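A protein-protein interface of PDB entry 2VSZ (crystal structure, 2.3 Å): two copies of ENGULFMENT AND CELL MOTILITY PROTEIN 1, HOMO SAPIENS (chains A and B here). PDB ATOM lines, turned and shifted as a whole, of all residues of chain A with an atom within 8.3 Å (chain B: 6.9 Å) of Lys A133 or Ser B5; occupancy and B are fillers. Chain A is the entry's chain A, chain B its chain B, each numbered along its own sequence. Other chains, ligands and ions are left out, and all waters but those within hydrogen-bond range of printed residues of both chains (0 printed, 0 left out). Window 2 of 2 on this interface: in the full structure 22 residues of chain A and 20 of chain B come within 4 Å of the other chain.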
ATOM      1  N   GLU A 110      26.412 -19.478   0.192  1.00  0.00           N
ATOM      2  CA  GLU A 110      25.639 -19.133   1.390  1.00  0.00           C
ATOM      3  C   GLU A 110      24.346 -18.396   1.068  1.00  0.00           C
ATOM      4  O   GLU A 110      23.378 -18.553   1.772  1.00  0.00           O
ATOM      5  CB  GLU A 110      26.483 -18.324   2.402  1.00  0.00           C
ATOM      6  N   GLU A 113      21.658 -20.756  -0.313  1.00  0.00           N
ATOM      7  CA  GLU A 113      20.947 -21.470   0.760  1.00  0.00           C
ATOM      8  C   GLU A 113      19.812 -20.672   1.402  1.00  0.00           C
ATOM      9  O   GLU A 113      19.035 -21.217   2.143  1.00  0.00           O
ATOM     10  CB  GLU A 113      21.941 -22.009   1.786  1.00  0.00           C
ATOM     11  CG  GLU A 113      22.881 -23.049   1.138  1.00  0.00           C
ATOM     12  CD  GLU A 113      23.608 -24.005   2.083  1.00  0.00           C
ATOM     13  OE1 GLU A 113      23.132 -24.257   3.231  1.00  0.00           O
ATOM     14  OE2 GLU A 113      24.660 -24.560   1.637  1.00  0.00           O
ATOM     15  N   LEU A 114      19.710 -19.375   1.103  1.00  0.00           N
ATOM     16  CA  LEU A 114      18.771 -18.461   1.780  1.00  0.00           C
ATOM     17  C   LEU A 114      17.751 -17.916   0.823  1.00  0.00           C
ATOM     18  O   LEU A 114      16.867 -17.203   1.242  1.00  0.00           O
ATOM     19  CB  LEU A 114      19.536 -17.269   2.413  1.00  0.00           C
ATOM     20  CG  LEU A 114      20.500 -17.702   3.525  1.00  0.00           C
ATOM     21  CD1 LEU A 114      21.419 -16.574   3.974  1.00  0.00           C
ATOM     22  CD2 LEU A 114      19.744 -18.275   4.715  1.00  0.00           C
ATOM     23  N   ALA A 130      16.426 -14.774   2.772  1.00  0.00           N
ATOM     24  CA  ALA A 130      16.111 -14.833   4.195  1.00  0.00           C
ATOM     25  C   ALA A 130      17.288 -14.300   5.012  1.00  0.00           C
ATOM     26  O   ALA A 130      18.417 -14.494   4.640  1.00  0.00           O
ATOM     27  CB  ALA A 130      15.790 -16.241   4.612  1.00  0.00           C
ATOM     28  N   PRO A 131      17.008 -13.664   6.150  1.00  0.00           N
ATOM     29  CA  PRO A 131      18.108 -13.151   7.016  1.00  0.00           C
ATOM     30  C   PRO A 131      18.948 -14.258   7.618  1.00  0.00           C
ATOM     31  O   PRO A 131      20.068 -14.022   8.017  1.00  0.00           O
ATOM     32  CB  PRO A 131      17.363 -12.431   8.148  1.00  0.00           C
ATOM     33  CG  PRO A 131      15.874 -12.454   7.802  1.00  0.00           C
ATOM     34  CD  PRO A 131      15.657 -13.182   6.538  1.00  0.00           C
ATOM     35  N   ASP A 132      18.382 -15.447   7.794  1.00  0.00           N
ATOM     36  CA  ASP A 132      19.090 -16.566   8.398  1.00  0.00           C
ATOM     37  C   ASP A 132      18.327 -17.861   7.962  1.00  0.00           C
ATOM     38  O   ASP A 132      17.255 -17.771   7.439  1.00  0.00           O
ATOM     39  CB  ASP A 132      19.235 -16.421   9.951  1.00  0.00           C
ATOM     40  CG  ASP A 132      17.887 -16.298  10.687  1.00  0.00           C
ATOM     41  OD1 ASP A 132      17.639 -15.256  11.374  1.00  0.00           O
ATOM     42  OD2 ASP A 132      17.003 -17.194  10.553  1.00  0.00           O
ATOM     43  N   LYS A 133      18.934 -19.016   8.179  1.00  0.00           N
ATOM     44  CA  LYS A 133      18.455 -20.328   7.843  1.00  0.00           C
ATOM     45  C   LYS A 133      17.151 -20.688   8.624  1.00  0.00           C
ATOM     46  O   LYS A 133      16.316 -21.373   8.087  1.00  0.00           O
ATOM     47  CB  LYS A 133      19.579 -21.369   8.082  1.00  0.00           C
ATOM     48  CG  LYS A 133      19.722 -21.809   9.571  1.00  0.00           C
ATOM     49  CD  LYS A 133      21.097 -22.515   9.853  1.00  0.00           C
ATOM     50  CE  LYS A 133      21.159 -23.064  11.286  1.00  0.00           C
ATOM     51  NZ  LYS A 133      22.531 -23.629  11.630  1.00  0.00           N
ATOM     52  N   HIS A 134      16.941 -20.134   9.829  1.00  0.00           N
ATOM     53  CA  HIS A 134      15.684 -20.357  10.562  1.00  0.00           C
ATOM     54  C   HIS A 134      14.500 -19.685   9.899  1.00  0.00           C
ATOM     55  O   HIS A 134      13.434 -20.282   9.776  1.00  0.00           O
ATOM     56  CB  HIS A 134      15.837 -19.956  12.037  1.00  0.00           C
ATOM     57  CG  HIS A 134      17.008 -20.611  12.695  1.00  0.00           C
ATOM     58  ND1 HIS A 134      18.175 -19.931  13.051  1.00  0.00           N
ATOM     59  CD2 HIS A 134      17.191 -21.894  13.063  1.00  0.00           C
ATOM     60  CE1 HIS A 134      19.018 -20.785  13.620  1.00  0.00           C
ATOM     61  NE2 HIS A 134      18.454 -21.990  13.589  1.00  0.00           N
ATOM     62  N   GLU A 135      14.700 -18.470   9.406  1.00  0.00           N
ATOM     63  CA  GLU A 135      13.640 -17.696   8.734  1.00  0.00           C
ATOM     64  C   GLU A 135      13.372 -18.338   7.372  1.00  0.00           C
ATOM     65  O   GLU A 135      12.254 -18.342   6.924  1.00  0.00           O
ATOM     66  CB  GLU A 135      14.081 -16.189   8.524  1.00  0.00           C
ATOM     67  CG  GLU A 135      14.231 -15.310   9.826  1.00  0.00           C
ATOM     68  CD  GLU A 135      12.999 -15.332  10.746  1.00  0.00           C
ATOM     69  OE1 GLU A 135      13.188 -15.182  11.967  1.00  0.00           O
ATOM     70  OE2 GLU A 135      11.840 -15.485  10.289  1.00  0.00           O
ATOM     71  N   TYR A 136      14.444 -18.731   6.675  1.00  0.00           N
ATOM     72  CA  TYR A 136      14.340 -19.457   5.405  1.00  0.00           C
ATOM     73  C   TYR A 136      13.447 -20.703   5.544  1.00  0.00           C
ATOM     74  O   TYR A 136      12.536 -20.944   4.743  1.00  0.00           O
ATOM     75  CB  TYR A 136      15.725 -19.912   4.964  1.00  0.00           C
ATOM     76  CG  TYR A 136      15.702 -20.804   3.746  1.00  0.00           C
ATOM     77  CD1 TYR A 136      15.582 -20.229   2.476  1.00  0.00           C
ATOM     78  CD2 TYR A 136      15.783 -22.227   3.855  1.00  0.00           C
ATOM     79  CE1 TYR A 136      15.560 -20.998   1.326  1.00  0.00           C
ATOM     80  CE2 TYR A 136      15.742 -23.054   2.673  1.00  0.00           C
ATOM     81  CZ  TYR A 136      15.624 -22.392   1.407  1.00  0.00           C
ATOM     82  OH  TYR A 136      15.594 -23.064   0.186  1.00  0.00           O
ATOM     83  N   CYS A 137      13.730 -21.521   6.567  1.00  0.00           N
ATOM     84  CA  CYS A 137      12.951 -22.707   6.858  1.00  0.00           C
ATOM     85  C   CYS A 137      11.539 -22.375   7.237  1.00  0.00           C
ATOM     86  O   CYS A 137      10.617 -23.089   6.849  1.00  0.00           O
ATOM     87  CB  CYS A 137      13.617 -23.499   7.964  1.00  0.00           C
ATOM     88  SG  CYS A 137      15.005 -24.372   7.345  1.00  0.00           S
ATOM     89  N   ILE A 138      11.331 -21.297   7.994  1.00  0.00           N
ATOM     90  CA  ILE A 138       9.948 -20.886   8.290  1.00  0.00           C
ATOM     91  C   ILE A 138       9.135 -20.623   7.020  1.00  0.00           C
ATOM     92  O   ILE A 138       7.965 -21.007   6.941  1.00  0.00           O
ATOM     93  CB  ILE A 138       9.860 -19.631   9.213  1.00  0.00           C
ATOM     94  CG1 ILE A 138      10.368 -19.991  10.604  1.00  0.00           C
ATOM     95  CG2 ILE A 138       8.454 -18.909   9.073  1.00  0.00           C
ATOM     96  CD1 ILE A 138      10.616 -18.859  11.563  1.00  0.00           C
ATOM     97  N   TRP A 139       9.709 -19.898   6.073  1.00  0.00           N
ATOM     98  CA  TRP A 139       9.019 -19.598   4.791  1.00  0.00           C
ATOM     99  C   TRP A 139       8.847 -20.841   3.870  1.00  0.00           C
ATOM    100  O   TRP A 139       7.745 -21.114   3.378  1.00  0.00           O
ATOM    101  CB  TRP A 139       9.699 -18.367   4.070  1.00  0.00           C
ATOM    102  CG  TRP A 139       9.206 -17.193   4.825  1.00  0.00           C
ATOM    103  CD1 TRP A 139       9.794 -16.605   5.898  1.00  0.00           C
ATOM    104  CD2 TRP A 139       7.929 -16.550   4.652  1.00  0.00           C
ATOM    105  NE1 TRP A 139       8.962 -15.668   6.417  1.00  0.00           N
ATOM    106  CE2 TRP A 139       7.813 -15.603   5.668  1.00  0.00           C
ATOM    107  CE3 TRP A 139       6.835 -16.751   3.763  1.00  0.00           C
ATOM    108  CZ2 TRP A 139       6.681 -14.803   5.812  1.00  0.00           C
ATOM    109  CZ3 TRP A 139       5.672 -15.977   3.922  1.00  0.00           C
ATOM    110  CH2 TRP A 139       5.600 -15.022   4.936  1.00  0.00           C
ATOM    111  N   THR A 140       9.898 -21.609   3.664  1.00  0.00           N
ATOM    112  CA  THR A 140       9.768 -22.739   2.764  1.00  0.00           C
ATOM    113  C   THR A 140       8.858 -23.836   3.325  1.00  0.00           C
ATOM    114  O   THR A 140       7.973 -24.333   2.601  1.00  0.00           O
ATOM    115  CB  THR A 140      11.154 -23.312   2.275  1.00  0.00           C
ATOM    116  OG1 THR A 140      11.930 -23.692   3.398  1.00  0.00           O
ATOM    117  CG2 THR A 140      11.937 -22.269   1.385  1.00  0.00           C
ATOM    118  N   LEU B   3      24.276 -27.804   8.602  1.00  0.00           N
ATOM    119  CA  LEU B   3      23.363 -27.130   7.634  1.00  0.00           C
ATOM    120  C   LEU B   3      21.937 -27.570   7.938  1.00  0.00           C
ATOM    121  O   LEU B   3      21.701 -28.757   8.181  1.00  0.00           O
ATOM    122  CB  LEU B   3      23.754 -27.466   6.182  1.00  0.00           C
ATOM    123  CG  LEU B   3      25.224 -27.219   5.788  1.00  0.00           C
ATOM    124  CD1 LEU B   3      25.745 -28.394   4.923  1.00  0.00           C
ATOM    125  CD2 LEU B   3      25.505 -25.840   5.118  1.00  0.00           C
ATOM    126  N   GLY B   4      21.005 -26.611   7.977  1.00  0.00           N
ATOM    127  CA  GLY B   4      19.544 -26.903   8.103  1.00  0.00           C
ATOM    128  C   GLY B   4      18.885 -26.800   9.479  1.00  0.00           C
ATOM    129  O   GLY B   4      19.061 -27.696  10.341  1.00  0.00           O
ATOM    130  N   SER B   5      18.045 -25.771   9.625  1.00  0.00           N
ATOM    131  CA  SER B   5      17.297 -25.399  10.859  1.00  0.00           C
ATOM    132  C   SER B   5      16.414 -26.392  11.590  1.00  0.00           C
ATOM    133  O   SER B   5      15.633 -27.099  10.994  1.00  0.00           O
ATOM    134  CB  SER B   5      16.450 -24.134  10.620  1.00  0.00           C
ATOM    135  OG  SER B   5      15.640 -23.856  11.749  1.00  0.00           O
ATOM    136  N   PRO B   6      16.460 -26.367  12.934  1.00  0.00           N
ATOM    137  CA  PRO B   6      15.517 -27.120  13.780  1.00  0.00           C
ATOM    138  C   PRO B   6      14.018 -26.767  13.622  1.00  0.00           C
ATOM    139  O   PRO B   6      13.183 -27.441  14.181  1.00  0.00           O
ATOM    140  CB  PRO B   6      15.989 -26.758  15.206  1.00  0.00           C
ATOM    141  CG  PRO B   6      17.367 -26.385  15.041  1.00  0.00           C
ATOM    142  CD  PRO B   6      17.502 -25.720  13.740  1.00  0.00           C
ATOM    143  N   ILE B   7      13.681 -25.710  12.899  1.00  0.00           N
ATOM    144  CA  ILE B   7      12.319 -25.350  12.610  1.00  0.00           C
ATOM    145  C   ILE B   7      11.664 -26.436  11.728  1.00  0.00           C
ATOM    146  O   ILE B   7      10.453 -26.617  11.779  1.00  0.00           O
ATOM    147  CB  ILE B   7      12.311 -23.956  12.035  1.00  0.00           C
ATOM    148  CG1 ILE B   7      12.635 -22.986  13.200  1.00  0.00           C
ATOM    149  CG2 ILE B   7      11.051 -23.626  11.149  1.00  0.00           C
ATOM    150  CD1 ILE B   7      12.412 -21.659  12.929  1.00  0.00           C
ATOM    151  N   LEU B   8      12.480 -27.197  10.993  1.00  0.00           N
ATOM    152  CA  LEU B   8      12.007 -28.265  10.120  1.00  0.00           C
ATOM    153  C   LEU B   8      11.604 -29.521  10.813  1.00  0.00           C
ATOM    154  O   LEU B   8      10.917 -30.330  10.217  1.00  0.00           O
ATOM    155  CB  LEU B   8      13.098 -28.664   9.152  1.00  0.00           C
ATOM    156  CG  LEU B   8      12.984 -28.268   7.697  1.00  0.00           C
ATOM    157  CD1 LEU B   8      12.233 -26.940   7.446  1.00  0.00           C
ATOM    158  CD2 LEU B   8      14.390 -28.170   7.216  1.00  0.00           C
ATOM    159  N   GLU B   9      12.009 -29.720  12.060  1.00  0.00           N
ATOM    160  CA  GLU B   9      11.811 -31.023  12.694  1.00  0.00           C
ATOM    161  C   GLU B   9      10.369 -31.282  13.235  1.00  0.00           C
ATOM    162  O   GLU B   9      10.050 -32.353  13.725  1.00  0.00           O
ATOM    163  CB  GLU B   9      12.963 -31.311  13.696  1.00  0.00           C
ATOM    164  CG  GLU B   9      14.424 -31.293  13.043  1.00  0.00           C
ATOM    165  CD  GLU B   9      15.510 -30.888  14.052  1.00  0.00           C
ATOM    166  OE1 GLU B   9      15.150 -30.667  15.218  1.00  0.00           O
ATOM    167  OE2 GLU B   9      16.713 -30.726  13.718  1.00  0.00           O
ATOM    168  N   LYS B  13      10.667 -34.554  11.360  1.00  0.00           N
ATOM    169  CA  LYS B  13      11.068 -35.517  12.363  1.00  0.00           C
ATOM    170  C   LYS B  13       9.928 -35.922  13.336  1.00  0.00           C
ATOM    171  O   LYS B  13       9.604 -37.086  13.430  1.00  0.00           O
ATOM    172  CB  LYS B  13      12.392 -35.097  13.044  1.00  0.00           C
ATOM    173  CG  LYS B  13      13.644 -35.529  12.293  1.00  0.00           C
ATOM    174  CD  LYS B  13      14.899 -35.356  13.143  1.00  0.00           C
ATOM    175  CE  LYS B  13      15.497 -33.961  12.999  1.00  0.00           C
ATOM    176  NZ  LYS B  13      15.995 -33.717  11.619  1.00  0.00           N
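N of His A134 lies within hydrogen-bond range of OD2 of Asp A132 (3.0 Å). SG of Cys A137 is in hydrogen-bond range of O of Lys A133 (3.4 Å). N of Ile B7 is in hydrogen-bond range of OG of Ser B5.
Among the printed residues, pairs that only touch across the chains: Glu A113 with Leu B3, Lys A133 with Ser B5, His A134 with Ser B5, His A134 with Pro B6, His A134 with Ile B7, Cys A137 with Ser B5, Cys A137 with Leu B8 and Ile A138 with Ile B7.
Of chain B, only Ser B5 (3.7 Å) comes within 4 Å of Lys A133. Of the printed residues of chain A, Ser B5 touches Lys A133 (3.7 Å), His A134 (2.8 Å) and Cys A137 (3.6 Å). No residue of chain A comes within 4 Å of Gly B4. Printed residues of chain B within 4 Å of Ile A138: Ile B7 (3.5 Å). Printed residues of chain B within 4 Å of His A134: Ser B5, Pro B6 and Ile B7. Glu B9 touches none of the printed residues of chain A. Trp A139 touches none of the printed residues of chain B. The nearest residue of chain B that does not touch Lys A133 is Gly B4 (4.5 Å). The nearest printed residue of chain A that does not touch Ser B5 is Glu A135 (5.9 Å).
Printed residues of chain B that touch a printed residue of chain A: Leu B3, Ser B5, Pro B6, Ile B7 and Leu B8. Along chain B the printed residues that touch a printed residue of chain A span positions 3 to 8. Of the 14 printed residues of chain A, 5 touch a printed residue of chain B. Among the printed residues, 8 pairs touch across the chains. Among the printed residues, no Asp or Glu carboxylate lies within 4 Å of a Lys or Arg side-chain nitrogen of the other chain.
No position is printed for both chains.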
